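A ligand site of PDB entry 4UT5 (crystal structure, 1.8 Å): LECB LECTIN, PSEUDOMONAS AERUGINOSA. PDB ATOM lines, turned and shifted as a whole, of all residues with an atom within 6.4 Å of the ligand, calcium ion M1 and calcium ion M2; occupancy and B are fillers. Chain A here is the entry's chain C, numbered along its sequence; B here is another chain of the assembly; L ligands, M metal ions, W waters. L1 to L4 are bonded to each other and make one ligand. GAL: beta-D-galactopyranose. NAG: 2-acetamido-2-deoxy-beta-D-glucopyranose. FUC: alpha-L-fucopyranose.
The side-chain carboxylate of Asp 96 sits close to an oxygen (O2) of FUC L3 (2.5 Å). The backbone NH (N) of Ser 23 sits at hydrogen-bond distance from an oxygen (O5) of FUC L3 (3.1 Å). The side-chain hydroxyl of Ser 23 is in hydrogen-bond range of an oxygen (O5) of FUC L3 (3.4 Å). O5 of FUC L3 lies close to OG of Ser 22 (3.5 Å).
N of Asn 103 sits at hydrogen-bond distance from O of Ser 94 (3.5 Å). N of Asp 96 sits close to OD2 of Asp 104 (2.8 Å). The backbone NH (N) of Asp 104 is in hydrogen-bond range of the backbone carbonyl oxygen (O) of Ser 94 (3.1 Å). The side-chain carboxylate of Glu 95 sits close to the backbone NH of Asn 100 (3.2 Å). The side-chain carboxylate of Glu 95 lies close to the backbone NH of Tyr 102 (3.0 Å). The backbone NH of Gly 114 of chain B lies close to the backbone carbonyl oxygen of Thr 45, at 3.5 Å. The side-chain carboxylate (OD2) of Asp 96 sits at hydrogen-bond distance from the side-chain hydroxyl (OG) of Ser 22 (2.7 Å). OD2 of Asp 96 lies within hydrogen-bond range of NE2 of Gln 26 (2.9 Å).
Merely in contact with the ligand: Ser 97 (3.4 Å), Arg 72 (3.8 Å) and Ala 24 (3.98 Å). 12 residues have an atom within 4 Å of the ligand: Asn 21, Ser 22, Ser 23, Ala 24, Arg 72, Glu 95, Asp 96, Ser 97, Asp 99, Asp 101, Asp 104 and Gly 114 of chain B. Along chain A the residues within 4 Å of the ligand span positions 21 to 104.
Four residues have an atom within 4 Å of calcium ion M1: Glu 95, Asp 99, Asp 101 and Asp 104. Along chain A the residues within 4 Å of calcium ion M1 span positions 95 to 104.
Of the 21 residues printed, 5 come within 4 Å of calcium ion M2. The nearest printed residue that does not touch calcium ion M2 is Ser 22 (4.5 Å).
Calcium ion M1 is bound by the side-chain carboxylate (OD2) of Asp 104 (2.4 Å), the side-chain carboxylate (OD1) of Asp 99 (2.4 Å), the side-chain carboxylate (OE2) of Glu 95 (2.4 Å), the side-chain carboxylate (OD1) of Asp 101 (2.4 Å), an oxygen (O3) of FUC L3 (2.5 Å), the side-chain carboxylate (OE1) of Glu 95 (2.5 Å), an oxygen (O2) of FUC L3 (2.5 Å) and the side-chain carboxylate (OD1) of Asp 104 (2.7 Å).
OD1 of Asn 103 is bound to calcium ion M2, 2.3 Å away. Calcium ion M2 is bound by OD1 of Asp 104, 2.3 Å away. Calcium ion M2 is bound by the backbone carbonyl oxygen (O) of Asn 21 (2.5 Å). Calcium ion M2 is bound by O4 of FUC L3, at 2.5 Å. OD2 of Asp 101 binds calcium ion M2, 2.5 Å away. O3 of FUC L3 is bound to calcium ion M2. O of Gly 114 of chain B is bound to calcium ion M2 (2.5 Å). Slightly farther from calcium ion M2 lies the side-chain carboxylate (OD1) of Asp 101 (3.1 Å).
Water W5 bridges OG of Ser 23 and O3 of NAG L2. Water W2 lies within hydrogen-bond range of OG of Ser 97 (2.7 Å) and O6 of GAL L1 (3.0 Å).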
ATOM      1  N   ASN A  21      24.958   8.907  26.432  1.00  0.00           N
ATOM      2  CA  ASN A  21      24.184  10.150  26.123  1.00  0.00           C
ATOM      3  C   ASN A  21      23.103   9.897  25.107  1.00  0.00           C
ATOM      4  O   ASN A  21      23.256  10.235  23.920  1.00  0.00           O
ATOM      5  CB  ASN A  21      25.113  11.213  25.570  1.00  0.00           C
ATOM      6  CG  ASN A  21      26.104  11.708  26.592  1.00  0.00           C
ATOM      7  OD1 ASN A  21      25.778  12.497  27.434  1.00  0.00           O
ATOM      8  ND2 ASN A  21      27.325  11.245  26.496  1.00  0.00           N
ATOM      9  N   SER A  22      22.021   9.224  25.537  1.00  0.00           N
ATOM     10  CA  SER A  22      20.992   8.789  24.592  1.00  0.00           C
ATOM     11  C   SER A  22      19.785   8.372  25.412  1.00  0.00           C
ATOM     12  O   SER A  22      19.943   7.853  26.505  1.00  0.00           O
ATOM     13  CB  SER A  22      21.467   7.586  23.741  1.00  0.00           C
ATOM     14  OG  SER A  22      20.404   7.047  22.951  1.00  0.00           O
ATOM     15  N   SER A  23      18.598   8.458  24.818  1.00  0.00           N
ATOM     16  CA  SER A  23      17.429   7.947  25.510  1.00  0.00           C
ATOM     17  C   SER A  23      17.423   6.410  25.507  1.00  0.00           C
ATOM     18  O   SER A  23      16.714   5.782  26.283  1.00  0.00           O
ATOM     19  CB  SER A  23      16.130   8.534  24.860  1.00  0.00           C
ATOM     20  OG  SER A  23      16.012   8.101  23.526  1.00  0.00           O
ATOM     21  N   ALA A  24      18.210   5.794  24.628  1.00  0.00           N
ATOM     22  CA  ALA A  24      18.234   4.337  24.446  1.00  0.00           C
ATOM     23  C   ALA A  24      19.327   3.687  25.263  1.00  0.00           C
ATOM     24  O   ALA A  24      20.379   4.300  25.500  1.00  0.00           O
ATOM     25  CB  ALA A  24      18.400   4.000  23.011  1.00  0.00           C
ATOM     26  N   GLN A  26      22.369   1.569  26.042  1.00  0.00           N
ATOM     27  CA  GLN A  26      23.557   1.231  25.284  1.00  0.00           C
ATOM     28  C   GLN A  26      24.152  -0.054  25.818  1.00  0.00           C
ATOM     29  O   GLN A  26      24.265  -0.211  27.025  1.00  0.00           O
ATOM     30  CB  GLN A  26      24.616   2.342  25.479  1.00  0.00           C
ATOM     31  CG  GLN A  26      24.097   3.744  25.117  1.00  0.00           C
ATOM     32  CD  GLN A  26      23.778   3.896  23.644  1.00  0.00           C
ATOM     33  OE1 GLN A  26      24.627   3.638  22.778  1.00  0.00           O
ATOM     34  NE2 GLN A  26      22.521   4.323  23.322  1.00  0.00           N
ATOM     35  N   THR A  45      21.155  10.233  29.637  1.00  0.00           N
ATOM     36  CA  THR A  45      21.329  11.373  28.734  1.00  0.00           C
ATOM     37  C   THR A  45      22.224  12.449  29.406  1.00  0.00           C
ATOM     38  O   THR A  45      22.383  13.579  28.876  1.00  0.00           O
ATOM     39  CB  THR A  45      19.973  12.024  28.357  1.00  0.00           C
ATOM     40  OG1 THR A  45      19.215  12.220  29.570  1.00  0.00           O
ATOM     41  CG2 THR A  45      19.258  11.175  27.405  1.00  0.00           C
ATOM     42  N   VAL A  69      22.289  -1.171  20.348  1.00  0.00           N
ATOM     43  CA  VAL A  69      21.126  -0.693  21.082  1.00  0.00           C
ATOM     44  C   VAL A  69      20.020  -1.688  20.705  1.00  0.00           C
ATOM     45  O   VAL A  69      19.614  -1.746  19.545  1.00  0.00           O
ATOM     46  CB  VAL A  69      20.780   0.740  20.678  1.00  0.00           C
ATOM     47  CG1 VAL A  69      19.474   1.173  21.330  1.00  0.00           C
ATOM     48  CG2 VAL A  69      21.921   1.668  21.044  1.00  0.00           C
ATOM     49  N   ARG A  72      20.693  -3.734  17.553  1.00  0.00           N
ATOM     50  CA  ARG A  72      21.115  -3.048  16.315  1.00  0.00           C
ATOM     51  C   ARG A  72      22.496  -2.412  16.530  1.00  0.00           C
ATOM     52  O   ARG A  72      22.680  -1.613  17.461  1.00  0.00           O
ATOM     53  CB  ARG A  72      20.171  -1.963  15.829  1.00  0.00           C
ATOM     54  CG  ARG A  72      18.681  -2.213  15.982  1.00  0.00           C
ATOM     55  CD  ARG A  72      17.940  -0.957  15.515  1.00  0.00           C
ATOM     56  NE  ARG A  72      18.117   0.056  16.568  1.00  0.00           N
ATOM     57  CZ  ARG A  72      17.344   0.190  17.650  1.00  0.00           C
ATOM     58  NH1 ARG A  72      16.266  -0.571  17.831  1.00  0.00           N
ATOM     59  NH2 ARG A  72      17.639   1.117  18.560  1.00  0.00           N
ATOM     60  N   SER A  94      29.790   6.698  19.000  1.00  0.00           N
ATOM     61  CA  SER A  94      28.800   5.834  18.355  1.00  0.00           C
ATOM     62  C   SER A  94      27.463   6.555  18.245  1.00  0.00           C
ATOM     63  O   SER A  94      27.114   7.419  19.058  1.00  0.00           O
ATOM     64  CB  SER A  94      28.616   4.569  19.068  1.00  0.00           C
ATOM     65  OG  SER A  94      28.153   4.769  20.387  1.00  0.00           O
ATOM     66  N   GLU A  95      26.779   6.215  17.159  1.00  0.00           N
ATOM     67  CA  GLU A  95      25.507   6.878  16.759  1.00  0.00           C
ATOM     68  C   GLU A  95      24.439   5.806  16.599  1.00  0.00           C
ATOM     69  O   GLU A  95      24.581   4.870  15.781  1.00  0.00           O
ATOM     70  CB  GLU A  95      25.695   7.647  15.470  1.00  0.00           C
ATOM     71  CG  GLU A  95      24.449   8.350  14.943  1.00  0.00           C
ATOM     72  CD  GLU A  95      23.795   9.205  16.014  1.00  0.00           C
ATOM     73  OE1 GLU A  95      24.512  10.067  16.601  1.00  0.00           O
ATOM     74  OE2 GLU A  95      22.586   9.022  16.305  1.00  0.00           O
ATOM     75  N   ASP A  96      23.398   5.913  17.410  1.00  0.00           N
ATOM     76  CA  ASP A  96      22.320   4.913  17.431  1.00  0.00           C
ATOM     77  C   ASP A  96      21.104   5.389  16.610  1.00  0.00           C
ATOM     78  O   ASP A  96      20.073   4.697  16.591  1.00  0.00           O
ATOM     79  CB  ASP A  96      21.946   4.551  18.865  1.00  0.00           C
ATOM     80  CG  ASP A  96      21.346   5.705  19.679  1.00  0.00           C
ATOM     81  OD1 ASP A  96      20.779   6.691  19.083  1.00  0.00           O
ATOM     82  OD2 ASP A  96      21.403   5.625  20.924  1.00  0.00           O
ATOM     83  N   SER A  97      21.214   6.557  15.974  1.00  0.00           N
ATOM     84  CA  SER A  97      20.040   7.212  15.286  1.00  0.00           C
ATOM     85  C   SER A  97      20.491   8.105  14.160  1.00  0.00           C
ATOM     86  O   SER A  97      21.425   7.749  13.418  1.00  0.00           O
ATOM     87  CB  SER A  97      19.230   8.001  16.332  1.00  0.00           C
ATOM     88  OG  SER A  97      18.000   8.547  15.809  1.00  0.00           O
ATOM     89  N   THR A  98      19.833   9.239  13.975  1.00  0.00           N
ATOM     90  CA  THR A  98      19.993  10.063  12.778  1.00  0.00           C
ATOM     91  C   THR A  98      20.557  11.451  13.047  1.00  0.00           C
ATOM     92  O   THR A  98      20.859  12.165  12.094  1.00  0.00           O
ATOM     93  CB  THR A  98      18.623  10.249  12.082  1.00  0.00           C
ATOM     94  OG1 THR A  98      17.717  10.861  12.992  1.00  0.00           O
ATOM     95  CG2 THR A  98      18.062   8.883  11.620  1.00  0.00           C
ATOM     96  N   ASP A  99      20.720  11.848  14.305  1.00  0.00           N
ATOM     97  CA  ASP A  99      21.185  13.207  14.594  1.00  0.00           C
ATOM     98  C   ASP A  99      22.687  13.362  14.504  1.00  0.00           C
ATOM     99  O   ASP A  99      23.194  14.472  14.459  1.00  0.00           O
ATOM    100  CB  ASP A  99      20.661  13.712  15.948  1.00  0.00           C
ATOM    101  CG  ASP A  99      21.268  13.007  17.126  1.00  0.00           C
ATOM    102  OD1 ASP A  99      21.822  11.888  16.939  1.00  0.00           O
ATOM    103  OD2 ASP A  99      21.151  13.547  18.273  1.00  0.00           O
ATOM    104  N   ASN A 100      23.406  12.229  14.445  1.00  0.00           N
ATOM    105  CA  ASN A 100      24.843  12.269  14.225  1.00  0.00           C
ATOM    106  C   ASN A 100      25.641  13.092  15.199  1.00  0.00           C
ATOM    107  O   ASN A 100      26.714  13.691  14.829  1.00  0.00           O
ATOM    108  CB  ASN A 100      25.153  12.695  12.797  1.00  0.00           C
ATOM    109  CG  ASN A 100      24.573  11.744  11.777  1.00  0.00           C
ATOM    110  OD1 ASN A 100      24.321  10.585  12.066  1.00  0.00           O
ATOM    111  ND2 ASN A 100      24.353  12.240  10.570  1.00  0.00           N
ATOM    112  N   ASP A 101      25.246  13.052  16.478  1.00  0.00           N
ATOM    113  CA  ASP A 101      26.127  13.578  17.516  1.00  0.00           C
ATOM    114  C   ASP A 101      27.270  12.602  17.899  1.00  0.00           C
ATOM    115  O   ASP A 101      28.293  13.027  18.476  1.00  0.00           O
ATOM    116  CB  ASP A 101      25.374  14.150  18.778  1.00  0.00           C
ATOM    117  CG  ASP A 101      24.468  13.143  19.462  1.00  0.00           C
ATOM    118  OD1 ASP A 101      24.370  11.957  18.991  1.00  0.00           O
ATOM    119  OD2 ASP A 101      23.841  13.528  20.508  1.00  0.00           O
ATOM    120  N   TYR A 102      27.123  11.310  17.563  1.00  0.00           N
ATOM    121  CA  TYR A 102      28.147  10.311  17.851  1.00  0.00           C
ATOM    122  C   TYR A 102      28.550  10.247  19.320  1.00  0.00           C
ATOM    123  O   TYR A 102      29.663   9.800  19.643  1.00  0.00           O
ATOM    124  CB  TYR A 102      29.370  10.478  16.888  1.00  0.00           C
ATOM    125  CG  TYR A 102      29.050   9.900  15.520  1.00  0.00           C
ATOM    126  CD1 TYR A 102      29.203   8.569  15.264  1.00  0.00           C
ATOM    127  CD2 TYR A 102      28.450  10.699  14.554  1.00  0.00           C
ATOM    128  CE1 TYR A 102      28.869   8.052  14.023  1.00  0.00           C
ATOM    129  CE2 TYR A 102      28.101  10.166  13.310  1.00  0.00           C
ATOM    130  CZ  TYR A 102      28.288   8.860  13.082  1.00  0.00           C
ATOM    131  OH  TYR A 102      27.892   8.340  11.868  1.00  0.00           O
ATOM    132  N   ASN A 103      27.642  10.638  20.234  1.00  0.00           N
ATOM    133  CA  ASN A 103      27.947  10.622  21.636  1.00  0.00           C
ATOM    134  C   ASN A 103      27.090   9.608  22.427  1.00  0.00           C
ATOM    135  O   ASN A 103      27.112   9.606  23.651  1.00  0.00           O
ATOM    136  CB  ASN A 103      27.743  12.005  22.247  1.00  0.00           C
ATOM    137  CG  ASN A 103      26.299  12.385  22.385  1.00  0.00           C
ATOM    138  OD1 ASN A 103      25.434  11.649  21.942  1.00  0.00           O
ATOM    139  ND2 ASN A 103      26.027  13.523  23.003  1.00  0.00           N
ATOM    140  N   ASP A 104      26.330   8.800  21.708  1.00  0.00           N
ATOM    141  CA  ASP A 104      25.263   7.995  22.332  1.00  0.00           C
ATOM    142  C   ASP A 104      25.899   7.001  23.309  1.00  0.00           C
ATOM    143  O   ASP A 104      25.435   6.825  24.448  1.00  0.00           O
ATOM    144  CB  ASP A 104      24.444   7.340  21.274  1.00  0.00           C
ATOM    145  CG  ASP A 104      23.728   8.377  20.381  1.00  0.00           C
ATOM    146  OD1 ASP A 104      23.416   9.475  20.902  1.00  0.00           O
ATOM    147  OD2 ASP A 104      23.605   8.141  19.150  1.00  0.00           O
ATOM    148  N   LEU B 113      26.921  16.695  25.192  1.00  0.00           N
ATOM    149  CA  LEU B 113      26.245  15.650  25.968  1.00  0.00           C
ATOM    150  C   LEU B 113      24.800  15.500  25.429  1.00  0.00           C
ATOM    151  O   LEU B 113      24.377  16.266  24.565  1.00  0.00           O
ATOM    152  CB  LEU B 113      26.232  16.036  27.431  1.00  0.00           C
ATOM    153  CG  LEU B 113      27.586  16.289  28.049  1.00  0.00           C
ATOM    154  CD1 LEU B 113      27.450  16.447  29.534  1.00  0.00           C
ATOM    155  CD2 LEU B 113      28.573  15.181  27.696  1.00  0.00           C
ATOM    156  N   GLY B 114      24.074  14.565  25.997  1.00  0.00           N
ATOM    157  CA  GLY B 114      22.663  14.420  25.766  1.00  0.00           C
ATOM    158  C   GLY B 114      22.267  13.637  24.550  1.00  0.00           C
ATOM    159  O   GLY B 114      23.101  13.317  23.663  1.00  0.00           O
ATOM    160  OXT GLY B 114      21.059  13.216  24.479  1.00  0.00           O
HETATM  161  C1  GAL L   1      15.313  12.140  19.886  1.00  0.00           C
HETATM  162  C2  GAL L   1      15.024  13.084  21.040  1.00  0.00           C
HETATM  163  C3  GAL L   1      14.717  14.482  20.510  1.00  0.00           C
HETATM  164  C4  GAL L   1      15.790  14.910  19.516  1.00  0.00           C
HETATM  165  C5  GAL L   1      16.061  13.830  18.465  1.00  0.00           C
HETATM  166  C6  GAL L   1      17.095  14.237  17.407  1.00  0.00           C
HETATM  167  O2  GAL L   1      13.980  12.650  21.865  1.00  0.00           O
HETATM  168  O3  GAL L   1      14.769  15.286  21.639  1.00  0.00           O
HETATM  169  O4  GAL L   1      16.889  15.097  20.335  1.00  0.00           O
HETATM  170  O5  GAL L   1      16.428  12.633  19.158  1.00  0.00           O
HETATM  171  O6  GAL L   1      16.958  13.483  16.230  1.00  0.00           O
HETATM  172  C1  NAG L   2      14.518   7.807  18.373  1.00  0.00           C
HETATM  173  C2  NAG L   2      14.413   9.087  19.173  1.00  0.00           C
HETATM  174  C3  NAG L   2      15.699   9.845  19.412  1.00  0.00           C
HETATM  175  C4  NAG L   2      16.731   8.860  19.951  1.00  0.00           C
HETATM  176  C5  NAG L   2      16.721   7.504  19.263  1.00  0.00           C
HETATM  177  C6  NAG L   2      17.536   6.498  20.040  1.00  0.00           C
HETATM  178  C7  NAG L   2      12.115   9.887  19.040  1.00  0.00           C
HETATM  179  C8  NAG L   2      11.206  10.842  18.397  1.00  0.00           C
HETATM  180  N2  NAG L   2      13.416   9.942  18.587  1.00  0.00           N
HETATM  181  O3  NAG L   2      15.552  10.830  20.416  1.00  0.00           O
HETATM  182  O4  NAG L   2      17.969   9.455  19.677  1.00  0.00           O
HETATM  183  O5  NAG L   2      15.388   7.037  19.168  1.00  0.00           O
HETATM  184  O6  NAG L   2      17.344   5.261  19.391  1.00  0.00           O
HETATM  185  O7  NAG L   2      11.615   9.126  19.894  1.00  0.00           O
HETATM  186  C1  FUC L   3      18.856   9.269  20.795  1.00  0.00           C
HETATM  187  C2  FUC L   3      20.233   9.788  20.382  1.00  0.00           C
HETATM  188  C3  FUC L   3      20.204  11.297  20.235  1.00  0.00           C
HETATM  189  C4  FUC L   3      19.771  11.910  21.573  1.00  0.00           C
HETATM  190  C5  FUC L   3      18.421  11.276  22.001  1.00  0.00           C
HETATM  191  C6  FUC L   3      17.981  11.839  23.350  1.00  0.00           C
HETATM  192  O2  FUC L   3      20.655   9.207  19.148  1.00  0.00           O
HETATM  193  O3  FUC L   3      21.517  11.675  19.923  1.00  0.00           O
HETATM  194  O4  FUC L   3      20.812  11.637  22.567  1.00  0.00           O
HETATM  195  O5  FUC L   3      18.524   9.835  22.070  1.00  0.00           O
HETATM  196  C1  GAL L   4      11.674   5.062  15.633  1.00  0.00           C
HETATM  197  C2  GAL L   4      11.762   6.024  16.798  1.00  0.00           C
HETATM  198  C3  GAL L   4      13.216   6.199  17.244  1.00  0.00           C
HETATM  199  C4  GAL L   4      13.795   4.870  17.680  1.00  0.00           C
HETATM  200  C5  GAL L   4      13.546   3.871  16.536  1.00  0.00           C
HETATM  201  C6  GAL L   4      13.932   2.470  16.973  1.00  0.00           C
HETATM  202  O1  GAL L   4      10.313   4.820  15.376  1.00  0.00           O
HETATM  203  O2  GAL L   4      11.198   7.277  16.435  1.00  0.00           O
HETATM  204  O3  GAL L   4      13.266   7.148  18.277  1.00  0.00           O
HETATM  205  O4  GAL L   4      13.313   4.415  18.946  1.00  0.00           O
HETATM  206  O5  GAL L   4      12.203   3.835  16.037  1.00  0.00           O
HETATM  207  O6  GAL L   4      14.154   1.799  15.766  1.00  0.00           O
HETATM  208 CA    CA M   1      22.785  10.235  18.365  1.00  0.00          CA
HETATM  209 CA    CA M   2      23.165  11.538  21.842  1.00  0.00          CA
HETATM  210  O   HOH W   1       7.319   6.164  14.541  1.00  0.00           O
HETATM  211  O   HOH W   2      18.235  10.911  17.031  1.00  0.00           O
HETATM  212  O   HOH W   3      14.279  13.489  24.483  1.00  0.00           O
HETATM  213  O   HOH W   4      16.542  13.213  26.197  1.00  0.00           O
HETATM  214  O   HOH W   5      14.126   9.760  22.546  1.00  0.00           O
HETATM  215  O   HOH W   6      12.491   6.604  21.071  1.00  0.00           O
HETATM  216  O   HOH W   7      10.615   9.427  22.597  1.00  0.00           O
HETATM  217  O   HOH W   8      15.245   3.863  20.650  1.00  0.00           O
HETATM  218  O   HOH W   9      11.747  12.961  20.831  1.00  0.00           O
